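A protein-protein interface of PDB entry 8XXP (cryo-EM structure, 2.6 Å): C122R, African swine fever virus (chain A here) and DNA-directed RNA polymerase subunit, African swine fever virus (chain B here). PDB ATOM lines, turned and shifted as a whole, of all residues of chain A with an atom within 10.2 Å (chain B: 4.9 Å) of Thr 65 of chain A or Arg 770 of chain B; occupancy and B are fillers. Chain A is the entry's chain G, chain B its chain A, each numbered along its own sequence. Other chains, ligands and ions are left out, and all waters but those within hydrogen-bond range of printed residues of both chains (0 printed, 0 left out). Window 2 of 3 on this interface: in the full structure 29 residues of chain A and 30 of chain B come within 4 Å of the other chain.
Pro 61 of chain A touches none of the printed residues of chain B.
Of the printed residues of chain B, Asp 63 of chain A touches Arg 777 (2.3 Å).
Thr 65 of chain A touches three residues of chain B.
Of the printed residues of chain B, Cys 67 of chain A touches Pro 776 (3.7 Å) and Arg 777 (3.0 Å).
Gln 68 of chain A touches none of the printed residues of chain B.
No residue of chain A comes within 4 Å of Pro 764 of chain B.
No residue of chain A comes within 4 Å of Phe 766 of chain B.
No residue of chain A comes within 4 Å of Ser 767 of chain B.
Of the printed residues of chain A, Phe 768 of chain B touches Phe 56 (3.7 Å).
Gly 769 of chain B touches none of the printed residues of chain A.
Of the printed residues of chain A, Arg 770 of chain B touches Thr 65.
Thr 771 of chain B touches none of the printed residues of chain A.
No residue of chain A comes within 4 Å of Val 773 of chain B.
Printed residues of chain A within 4 Å of Arg 777 of chain B: Phe 56 (3.6 Å), Asp 63 (2.3 Å), Thr 65 (2.5 Å), Asn 66 (3.1 Å) and Cys 67 (3.0 Å).
Among the printed residues, merely in contact across the chains: Phe 56 of chain A with Phe 768 of chain B, Phe 56 of chain A with Arg 777 of chain B, Thr 65 of chain A with Arg 770 of chain B, Thr 65 of chain A with Pro 776 of chain B and Cys 67 of chain A with Pro 776 of chain B.
O of Arg 777 of chain B sits at hydrogen-bond distance from N of Cys 67 of chain A, 3.0 Å away.
The side-chain carboxylate of Asp 63 of chain A is in salt-bridge range of the guanidinium group of Arg 777 of chain B, at 3.8 Å.
The backbone NH (N) of Arg 777 of chain B is in hydrogen-bond range of the backbone carbonyl oxygen (O) of Thr 65 of chain A, 2.5 Å away.
The guanidinium group (NH1) of Arg 777 of chain B lies close to the side-chain amide oxygen (OD1) of Asn 66 of chain A, at 3.2 Å.
N of Gln 765 of chain B sits at hydrogen-bond distance from O of Arg 770 of chain B (3.4 Å).
The side-chain amide nitrogen (ND2) of Asn 66 of chain A lies within hydrogen-bond range of the backbone carbonyl oxygen (O) of Ala 60 of chain A, 3.2 Å away.
The side-chain carboxylate of Asp 63 of chain A lies within hydrogen-bond range of the side-chain hydroxyl of Thr 65 of chain A (3.0 Å).
The guanidinium group of Arg 770 of chain B sits at hydrogen-bond distance from the backbone carbonyl oxygen of Val 773 of chain B (3.1 Å).
The backbone carbonyl oxygen (O) of Tyr 775 of chain B is in hydrogen-bond range of the guanidinium group (NE) of Arg 770 of chain B, at 3.1 Å.
The guanidinium group of Arg 777 of chain B is in hydrogen-bond range of the backbone carbonyl oxygen of Phe 768 of chain B, at 2.9 Å.
Printed residues of chain B that touch a printed residue of chain A: Phe 768, Arg 770, Pro 776 and Arg 777.
Printed residues of chain A that touch a printed residue of chain B: Phe 56, Asp 63, Thr 65, Asn 66 and Cys 67.
Hydrophobic or aromatic side chains of chain A within 4 Å of the printed part of chain B: Phe 56.
Among the printed residues, Asp or Glu carboxylates within 4 Å of a Lys or Arg side-chain nitrogen of the other chain: Asp 63 of chain A with Arg 777 of chain B (2.3 Å).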
ATOM      1  N   PHE A  56      10.468  -4.204   8.443  1.00  0.00           N
ATOM      2  CA  PHE A  56      10.140  -3.758   7.093  1.00  0.00           C
ATOM      3  C   PHE A  56      10.990  -2.568   6.679  1.00  0.00           C
ATOM      4  O   PHE A  56      11.465  -2.506   5.544  1.00  0.00           O
ATOM      5  CB  PHE A  56       8.659  -3.404   6.995  1.00  0.00           C
ATOM      6  CG  PHE A  56       8.269  -2.830   5.666  1.00  0.00           C
ATOM      7  CD1 PHE A  56       8.138  -3.643   4.557  1.00  0.00           C
ATOM      8  CD2 PHE A  56       8.052  -1.473   5.520  1.00  0.00           C
ATOM      9  CE1 PHE A  56       7.789  -3.120   3.338  1.00  0.00           C
ATOM     10  CE2 PHE A  56       7.704  -0.946   4.299  1.00  0.00           C
ATOM     11  CZ  PHE A  56       7.572  -1.772   3.208  1.00  0.00           C
ATOM     12  N   ASN A  59      14.427  -3.686   5.894  1.00  0.00           N
ATOM     13  CA  ASN A  59      14.473  -4.428   4.639  1.00  0.00           C
ATOM     14  C   ASN A  59      14.158  -3.576   3.419  1.00  0.00           C
ATOM     15  O   ASN A  59      14.423  -4.011   2.298  1.00  0.00           O
ATOM     16  CB  ASN A  59      13.486  -5.590   4.691  1.00  0.00           C
ATOM     17  CG  ASN A  59      13.943  -6.696   5.598  1.00  0.00           C
ATOM     18  OD1 ASN A  59      15.124  -6.815   5.898  1.00  0.00           O
ATOM     19  ND2 ASN A  59      13.004  -7.516   6.046  1.00  0.00           N
ATOM     20  N   ALA A  60      13.588  -2.391   3.614  1.00  0.00           N
ATOM     21  CA  ALA A  60      13.150  -1.572   2.486  1.00  0.00           C
ATOM     22  C   ALA A  60      14.230  -1.274   1.453  1.00  0.00           C
ATOM     23  O   ALA A  60      13.925  -1.361   0.252  1.00  0.00           O
ATOM     24  CB  ALA A  60      12.541  -0.269   3.013  1.00  0.00           C
ATOM     25  N   PRO A  61      15.468  -0.922   1.809  1.00  0.00           N
ATOM     26  CA  PRO A  61      16.459  -0.630   0.761  1.00  0.00           C
ATOM     27  C   PRO A  61      16.763  -1.811  -0.135  1.00  0.00           C
ATOM     28  O   PRO A  61      17.361  -1.623  -1.201  1.00  0.00           O
ATOM     29  CB  PRO A  61      17.700  -0.204   1.552  1.00  0.00           C
ATOM     30  CG  PRO A  61      17.205   0.160   2.883  1.00  0.00           C
ATOM     31  CD  PRO A  61      16.024  -0.693   3.151  1.00  0.00           C
ATOM     32  N   PHE A  62      16.391  -3.023   0.267  1.00  0.00           N
ATOM     33  CA  PHE A  62      16.689  -4.226  -0.490  1.00  0.00           C
ATOM     34  C   PHE A  62      15.474  -4.812  -1.186  1.00  0.00           C
ATOM     35  O   PHE A  62      15.635  -5.665  -2.061  1.00  0.00           O
ATOM     36  CB  PHE A  62      17.317  -5.273   0.432  1.00  0.00           C
ATOM     37  CG  PHE A  62      18.497  -4.760   1.189  1.00  0.00           C
ATOM     38  CD1 PHE A  62      19.766  -4.856   0.657  1.00  0.00           C
ATOM     39  CD2 PHE A  62      18.337  -4.154   2.421  1.00  0.00           C
ATOM     40  CE1 PHE A  62      20.853  -4.374   1.343  1.00  0.00           C
ATOM     41  CE2 PHE A  62      19.422  -3.666   3.109  1.00  0.00           C
ATOM     42  CZ  PHE A  62      20.681  -3.778   2.570  1.00  0.00           C
ATOM     43  N   ASP A  63      14.281  -4.377  -0.835  1.00  0.00           N
ATOM     44  CA  ASP A  63      13.089  -4.832  -1.529  1.00  0.00           C
ATOM     45  C   ASP A  63      13.017  -4.157  -2.891  1.00  0.00           C
ATOM     46  O   ASP A  63      12.959  -2.922  -2.957  1.00  0.00           O
ATOM     47  CB  ASP A  63      11.853  -4.511  -0.702  1.00  0.00           C
ATOM     48  CG  ASP A  63      10.638  -5.286  -1.144  1.00  0.00           C
ATOM     49  OD1 ASP A  63      10.677  -5.891  -2.232  1.00  0.00           O
ATOM     50  OD2 ASP A  63       9.636  -5.291  -0.404  1.00  0.00           O
ATOM     51  N   PRO A  64      13.022  -4.908  -3.996  1.00  0.00           N
ATOM     52  CA  PRO A  64      12.950  -4.273  -5.317  1.00  0.00           C
ATOM     53  C   PRO A  64      11.568  -3.768  -5.682  1.00  0.00           C
ATOM     54  O   PRO A  64      11.434  -3.077  -6.699  1.00  0.00           O
ATOM     55  CB  PRO A  64      13.391  -5.397  -6.261  1.00  0.00           C
ATOM     56  CG  PRO A  64      12.997  -6.638  -5.558  1.00  0.00           C
ATOM     57  CD  PRO A  64      13.185  -6.368  -4.094  1.00  0.00           C
ATOM     58  N   THR A  65      10.548  -4.081  -4.893  1.00  0.00           N
ATOM     59  CA  THR A  65       9.186  -3.650  -5.166  1.00  0.00           C
ATOM     60  C   THR A  65       8.819  -2.348  -4.479  1.00  0.00           C
ATOM     61  O   THR A  65       7.674  -1.908  -4.599  1.00  0.00           O
ATOM     62  CB  THR A  65       8.196  -4.732  -4.741  1.00  0.00           C
ATOM     63  OG1 THR A  65       8.105  -4.758  -3.315  1.00  0.00           O
ATOM     64  CG2 THR A  65       8.660  -6.071  -5.220  1.00  0.00           C
ATOM     65  N   ASN A  66       9.747  -1.726  -3.761  1.00  0.00           N
ATOM     66  CA  ASN A  66       9.461  -0.476  -3.078  1.00  0.00           C
ATOM     67  C   ASN A  66       9.701   0.711  -4.000  1.00  0.00           C
ATOM     68  O   ASN A  66      10.635   0.722  -4.805  1.00  0.00           O
ATOM     69  CB  ASN A  66      10.324  -0.333  -1.827  1.00  0.00           C
ATOM     70  CG  ASN A  66       9.812  -1.156  -0.676  1.00  0.00           C
ATOM     71  OD1 ASN A  66       8.615  -1.369  -0.541  1.00  0.00           O
ATOM     72  ND2 ASN A  66      10.718  -1.613   0.173  1.00  0.00           N
ATOM     73  N   CYS A  67       8.840   1.716  -3.871  1.00  0.00           N
ATOM     74  CA  CYS A  67       8.981   2.933  -4.655  1.00  0.00           C
ATOM     75  C   CYS A  67      10.250   3.673  -4.256  1.00  0.00           C
ATOM     76  O   CYS A  67      10.645   3.679  -3.089  1.00  0.00           O
ATOM     77  CB  CYS A  67       7.761   3.831  -4.462  1.00  0.00           C
ATOM     78  SG  CYS A  67       7.907   5.479  -5.175  1.00  0.00           S
ATOM     79  N   GLN A  68      10.899   4.284  -5.238  1.00  0.00           N
ATOM     80  CA  GLN A  68      12.123   5.034  -5.014  1.00  0.00           C
ATOM     81  C   GLN A  68      11.993   6.411  -5.640  1.00  0.00           C
ATOM     82  O   GLN A  68      11.273   6.597  -6.622  1.00  0.00           O
ATOM     83  CB  GLN A  68      13.337   4.310  -5.590  1.00  0.00           C
ATOM     84  CG  GLN A  68      13.340   2.828  -5.303  1.00  0.00           C
ATOM     85  CD  GLN A  68      14.724   2.252  -5.297  1.00  0.00           C
ATOM     86  OE1 GLN A  68      15.606   2.735  -5.998  1.00  0.00           O
ATOM     87  NE2 GLN A  68      14.930   1.216  -4.501  1.00  0.00           N
ATOM     88  N   THR A  82      15.052   5.034  -1.234  1.00  0.00           N
ATOM     89  CA  THR A  82      13.814   4.276  -1.137  1.00  0.00           C
ATOM     90  C   THR A  82      12.796   5.046  -0.312  1.00  0.00           C
ATOM     91  O   THR A  82      13.074   5.425   0.827  1.00  0.00           O
ATOM     92  CB  THR A  82      14.069   2.909  -0.508  1.00  0.00           C
ATOM     93  OG1 THR A  82      15.064   2.215  -1.268  1.00  0.00           O
ATOM     94  CG2 THR A  82      12.790   2.097  -0.489  1.00  0.00           C
ATOM     95  N   GLN A  83      11.616   5.265  -0.875  1.00  0.00           N
ATOM     96  CA  GLN A  83      10.575   6.036  -0.210  1.00  0.00           C
ATOM     97  C   GLN A  83       9.521   5.101   0.364  1.00  0.00           C
ATOM     98  O   GLN A  83       9.031   4.209  -0.334  1.00  0.00           O
ATOM     99  CB  GLN A  83       9.928   7.026  -1.175  1.00  0.00           C
ATOM    100  CG  GLN A  83       8.700   7.700  -0.604  1.00  0.00           C
ATOM    101  CD  GLN A  83       7.634   7.940  -1.644  1.00  0.00           C
ATOM    102  OE1 GLN A  83       7.799   8.769  -2.539  1.00  0.00           O
ATOM    103  NE2 GLN A  83       6.532   7.213  -1.536  1.00  0.00           N
ATOM    104  N   ILE A  84       9.171   5.314   1.628  1.00  0.00           N
ATOM    105  CA  ILE A  84       8.211   4.483   2.344  1.00  0.00           C
ATOM    106  C   ILE A  84       7.137   5.385   2.928  1.00  0.00           C
ATOM    107  O   ILE A  84       7.451   6.376   3.591  1.00  0.00           O
ATOM    108  CB  ILE A  84       8.887   3.670   3.463  1.00  0.00           C
ATOM    109  CG1 ILE A  84       9.925   2.720   2.883  1.00  0.00           C
ATOM    110  CG2 ILE A  84       7.866   2.908   4.271  1.00  0.00           C
ATOM    111  CD1 ILE A  84      11.327   3.141   3.182  1.00  0.00           C
ATOM    112  N   CYS A  85       5.879   5.039   2.695  1.00  0.00           N
ATOM    113  CA  CYS A  85       4.749   5.748   3.285  1.00  0.00           C
ATOM    114  C   CYS A  85       3.954   4.752   4.115  1.00  0.00           C
ATOM    115  O   CYS A  85       3.215   3.932   3.565  1.00  0.00           O
ATOM    116  CB  CYS A  85       3.879   6.387   2.207  1.00  0.00           C
ATOM    117  SG  CYS A  85       2.446   7.261   2.839  1.00  0.00           S
ATOM    118  N   ARG A  97      20.532   1.759   1.318  1.00  0.00           N
ATOM    119  CA  ARG A  97      21.191   0.495   1.618  1.00  0.00           C
ATOM    120  C   ARG A  97      22.288   0.675   2.654  1.00  0.00           C
ATOM    121  O   ARG A  97      22.480  -0.185   3.522  1.00  0.00           O
ATOM    122  CB  ARG A  97      21.760  -0.116   0.338  1.00  0.00           C
ATOM    123  CG  ARG A  97      21.128   0.416  -0.935  1.00  0.00           C
ATOM    124  CD  ARG A  97      21.795  -0.167  -2.165  1.00  0.00           C
ATOM    125  NE  ARG A  97      21.985  -1.608  -2.053  1.00  0.00           N
ATOM    126  CZ  ARG A  97      21.043  -2.514  -2.278  1.00  0.00           C
ATOM    127  NH1 ARG A  97      19.813  -2.164  -2.617  1.00  0.00           N
ATOM    128  NH2 ARG A  97      21.342  -3.805  -2.156  1.00  0.00           N
ATOM    129  N   GLN B 763      -7.836   0.377  -3.732  1.00  0.00           N
ATOM    130  CA  GLN B 763      -7.135   0.115  -2.489  1.00  0.00           C
ATOM    131  C   GLN B 763      -5.981  -0.856  -2.713  1.00  0.00           C
ATOM    132  O   GLN B 763      -6.101  -1.806  -3.490  1.00  0.00           O
ATOM    133  CB  GLN B 763      -8.090  -0.457  -1.448  1.00  0.00           C
ATOM    134  CG  GLN B 763      -9.064   0.559  -0.870  1.00  0.00           C
ATOM    135  CD  GLN B 763      -8.475   1.951  -0.779  1.00  0.00           C
ATOM    136  OE1 GLN B 763      -8.939   2.878  -1.441  1.00  0.00           O
ATOM    137  NE2 GLN B 763      -7.452   2.106   0.050  1.00  0.00           N
ATOM    138  N   PRO B 764      -4.858  -0.649  -2.038  1.00  0.00           N
ATOM    139  CA  PRO B 764      -3.719  -1.551  -2.225  1.00  0.00           C
ATOM    140  C   PRO B 764      -3.957  -2.916  -1.604  1.00  0.00           C
ATOM    141  O   PRO B 764      -3.484  -3.202  -0.501  1.00  0.00           O
ATOM    142  CB  PRO B 764      -2.566  -0.805  -1.544  1.00  0.00           C
ATOM    143  CG  PRO B 764      -3.215   0.080  -0.567  1.00  0.00           C
ATOM    144  CD  PRO B 764      -4.527   0.485  -1.161  1.00  0.00           C
ATOM    145  N   GLN B 765      -4.692  -3.768  -2.318  1.00  0.00           N
ATOM    146  CA  GLN B 765      -5.023  -5.104  -1.850  1.00  0.00           C
ATOM    147  C   GLN B 765      -4.121  -6.191  -2.414  1.00  0.00           C
ATOM    148  O   GLN B 765      -4.181  -7.326  -1.936  1.00  0.00           O
ATOM    149  CB  GLN B 765      -6.480  -5.435  -2.194  1.00  0.00           C
ATOM    150  CG  GLN B 765      -7.471  -5.032  -1.125  1.00  0.00           C
ATOM    151  CD  GLN B 765      -7.086  -5.548   0.248  1.00  0.00           C
ATOM    152  OE1 GLN B 765      -7.253  -6.730   0.550  1.00  0.00           O
ATOM    153  NE2 GLN B 765      -6.565  -4.660   1.086  1.00  0.00           N
ATOM    154  N   PHE B 766      -3.301  -5.885  -3.420  1.00  0.00           N
ATOM    155  CA  PHE B 766      -2.394  -6.892  -3.959  1.00  0.00           C
ATOM    156  C   PHE B 766      -1.394  -7.340  -2.907  1.00  0.00           C
ATOM    157  O   PHE B 766      -1.145  -8.539  -2.740  1.00  0.00           O
ATOM    158  CB  PHE B 766      -1.665  -6.338  -5.180  1.00  0.00           C
ATOM    159  CG  PHE B 766      -0.534  -7.197  -5.655  1.00  0.00           C
ATOM    160  CD1 PHE B 766      -0.775  -8.413  -6.261  1.00  0.00           C
ATOM    161  CD2 PHE B 766       0.772  -6.789  -5.490  1.00  0.00           C
ATOM    162  CE1 PHE B 766       0.265  -9.198  -6.695  1.00  0.00           C
ATOM    163  CE2 PHE B 766       1.810  -7.573  -5.921  1.00  0.00           C
ATOM    164  CZ  PHE B 766       1.557  -8.775  -6.525  1.00  0.00           C
ATOM    165  N   SER B 767      -0.820  -6.387  -2.187  1.00  0.00           N
ATOM    166  CA  SER B 767       0.168  -6.646  -1.159  1.00  0.00           C
ATOM    167  C   SER B 767       0.060  -5.522  -0.140  1.00  0.00           C
ATOM    168  O   SER B 767      -0.905  -4.754  -0.141  1.00  0.00           O
ATOM    169  CB  SER B 767       1.568  -6.753  -1.771  1.00  0.00           C
ATOM    170  OG  SER B 767       2.483  -7.314  -0.854  1.00  0.00           O
ATOM    171  N   PHE B 768       1.047  -5.427   0.739  1.00  0.00           N
ATOM    172  CA  PHE B 768       1.102  -4.308   1.669  1.00  0.00           C
ATOM    173  C   PHE B 768       1.544  -3.065   0.912  1.00  0.00           C
ATOM    174  O   PHE B 768       2.715  -2.934   0.556  1.00  0.00           O
ATOM    175  CB  PHE B 768       2.053  -4.618   2.819  1.00  0.00           C
ATOM    176  CG  PHE B 768       2.429  -3.413   3.627  1.00  0.00           C
ATOM    177  CD1 PHE B 768       1.458  -2.645   4.241  1.00  0.00           C
ATOM    178  CD2 PHE B 768       3.752  -3.039   3.757  1.00  0.00           C
ATOM    179  CE1 PHE B 768       1.797  -1.536   4.970  1.00  0.00           C
ATOM    180  CE2 PHE B 768       4.095  -1.931   4.492  1.00  0.00           C
ATOM    181  CZ  PHE B 768       3.116  -1.176   5.096  1.00  0.00           C
ATOM    182  N   GLY B 769       0.609  -2.158   0.650  1.00  0.00           N
ATOM    183  CA  GLY B 769       0.937  -0.926  -0.032  1.00  0.00           C
ATOM    184  C   GLY B 769       1.022  -1.014  -1.536  1.00  0.00           C
ATOM    185  O   GLY B 769       1.515  -0.073  -2.164  1.00  0.00           O
ATOM    186  N   ARG B 770       0.557  -2.107  -2.135  1.00  0.00           N
ATOM    187  CA  ARG B 770       0.616  -2.316  -3.575  1.00  0.00           C
ATOM    188  C   ARG B 770      -0.783  -2.569  -4.110  1.00  0.00           C
ATOM    189  O   ARG B 770      -1.510  -3.406  -3.572  1.00  0.00           O
ATOM    190  CB  ARG B 770       1.514  -3.499  -3.924  1.00  0.00           C
ATOM    191  CG  ARG B 770       2.952  -3.320  -3.542  1.00  0.00           C
ATOM    192  CD  ARG B 770       3.784  -4.447  -4.082  1.00  0.00           C
ATOM    193  NE  ARG B 770       4.057  -4.280  -5.500  1.00  0.00           N
ATOM    194  CZ  ARG B 770       4.674  -5.177  -6.252  1.00  0.00           C
ATOM    195  NH1 ARG B 770       5.061  -6.339  -5.761  1.00  0.00           N
ATOM    196  NH2 ARG B 770       4.914  -4.898  -7.526  1.00  0.00           N
ATOM    197  N   THR B 771      -1.151  -1.858  -5.172  1.00  0.00           N
ATOM    198  CA  THR B 771      -2.426  -2.103  -5.833  1.00  0.00           C
ATOM    199  C   THR B 771      -2.330  -3.212  -6.871  1.00  0.00           C
ATOM    200  O   THR B 771      -3.278  -3.981  -7.038  1.00  0.00           O
ATOM    201  CB  THR B 771      -2.938  -0.825  -6.498  1.00  0.00           C
ATOM    202  OG1 THR B 771      -1.895  -0.252  -7.293  1.00  0.00           O
ATOM    203  CG2 THR B 771      -3.379   0.180  -5.461  1.00  0.00           C
ATOM    204  N   LEU B 772      -1.206  -3.299  -7.576  1.00  0.00           N
ATOM    205  CA  LEU B 772      -0.990  -4.319  -8.590  1.00  0.00           C
ATOM    206  C   LEU B 772       0.488  -4.667  -8.605  1.00  0.00           C
ATOM    207  O   LEU B 772       1.312  -3.975  -8.008  1.00  0.00           O
ATOM    208  CB  LEU B 772      -1.434  -3.849  -9.979  1.00  0.00           C
ATOM    209  CG  LEU B 772      -2.919  -3.758 -10.314  1.00  0.00           C
ATOM    210  CD1 LEU B 772      -3.083  -3.297 -11.738  1.00  0.00           C
ATOM    211  CD2 LEU B 772      -3.608  -5.083 -10.101  1.00  0.00           C
ATOM    212  N   VAL B 773       0.819  -5.756  -9.298  1.00  0.00           N
ATOM    213  CA  VAL B 773       2.213  -6.142  -9.479  1.00  0.00           C
ATOM    214  C   VAL B 773       2.954  -5.210 -10.420  1.00  0.00           C
ATOM    215  O   VAL B 773       4.185  -5.247 -10.480  1.00  0.00           O
ATOM    216  CB  VAL B 773       2.300  -7.594  -9.990  1.00  0.00           C
ATOM    217  CG1 VAL B 773       2.047  -7.648 -11.476  1.00  0.00           C
ATOM    218  CG2 VAL B 773       3.645  -8.203  -9.650  1.00  0.00           C
ATOM    219  N   TYR B 774       2.233  -4.369 -11.153  1.00  0.00           N
ATOM    220  CA  TYR B 774       2.834  -3.441 -12.092  1.00  0.00           C
ATOM    221  C   TYR B 774       3.257  -2.138 -11.447  1.00  0.00           C
ATOM    222  O   TYR B 774       3.904  -1.319 -12.103  1.00  0.00           O
ATOM    223  CB  TYR B 774       1.855  -3.151 -13.229  1.00  0.00           C
ATOM    224  CG  TYR B 774       1.409  -4.397 -13.936  1.00  0.00           C
ATOM    225  CD1 TYR B 774       2.338  -5.275 -14.462  1.00  0.00           C
ATOM    226  CD2 TYR B 774       0.068  -4.706 -14.066  1.00  0.00           C
ATOM    227  CE1 TYR B 774       1.953  -6.412 -15.100  1.00  0.00           C
ATOM    228  CE2 TYR B 774      -0.329  -5.847 -14.709  1.00  0.00           C
ATOM    229  CZ  TYR B 774       0.623  -6.699 -15.223  1.00  0.00           C
ATOM    230  OH  TYR B 774       0.243  -7.849 -15.868  1.00  0.00           O
ATOM    231  N   TYR B 775       2.925  -1.936 -10.180  1.00  0.00           N
ATOM    232  CA  TYR B 775       3.208  -0.691  -9.513  1.00  0.00           C
ATOM    233  C   TYR B 775       4.019  -0.945  -8.253  1.00  0.00           C
ATOM    234  O   TYR B 775       3.811  -1.957  -7.579  1.00  0.00           O
ATOM    235  CB  TYR B 775       1.907   0.033  -9.163  1.00  0.00           C
ATOM    236  CG  TYR B 775       1.100   0.382 -10.386  1.00  0.00           C
ATOM    237  CD1 TYR B 775       1.576   1.296 -11.312  1.00  0.00           C
ATOM    238  CD2 TYR B 775      -0.127  -0.214 -10.625  1.00  0.00           C
ATOM    239  CE1 TYR B 775       0.857   1.610 -12.426  1.00  0.00           C
ATOM    240  CE2 TYR B 775      -0.855   0.097 -11.741  1.00  0.00           C
ATOM    241  CZ  TYR B 775      -0.358   1.013 -12.639  1.00  0.00           C
ATOM    242  OH  TYR B 775      -1.075   1.338 -13.761  1.00  0.00           O
ATOM    243  N   PRO B 776       4.957  -0.065  -7.922  1.00  0.00           N
ATOM    244  CA  PRO B 776       5.793  -0.289  -6.745  1.00  0.00           C
ATOM    245  C   PRO B 776       5.001  -0.107  -5.464  1.00  0.00           C
ATOM    246  O   PRO B 776       3.872   0.383  -5.455  1.00  0.00           O
ATOM    247  CB  PRO B 776       6.880   0.775  -6.879  1.00  0.00           C
ATOM    248  CG  PRO B 776       6.237   1.849  -7.641  1.00  0.00           C
ATOM    249  CD  PRO B 776       5.312   1.182  -8.612  1.00  0.00           C
ATOM    250  N   ARG B 777       5.611  -0.536  -4.370  1.00  0.00           N
ATOM    251  CA  ARG B 777       4.999  -0.359  -3.064  1.00  0.00           C
ATOM    252  C   ARG B 777       5.012   1.110  -2.673  1.00  0.00           C
ATOM    253  O   ARG B 777       6.025   1.797  -2.822  1.00  0.00           O
ATOM    254  CB  ARG B 777       5.737  -1.194  -2.027  1.00  0.00           C
ATOM    255  CG  ARG B 777       5.030  -1.289  -0.714  1.00  0.00           C
ATOM    256  CD  ARG B 777       5.721  -2.265   0.201  1.00  0.00           C
ATOM    257  NE  ARG B 777       5.401  -3.643  -0.142  1.00  0.00           N
ATOM    258  CZ  ARG B 777       6.302  -4.599  -0.299  1.00  0.00           C
ATOM    259  NH1 ARG B 777       7.592  -4.362  -0.151  1.00  0.00           N
ATOM    260  NH2 ARG B 777       5.896  -5.825  -0.608  1.00  0.00           N
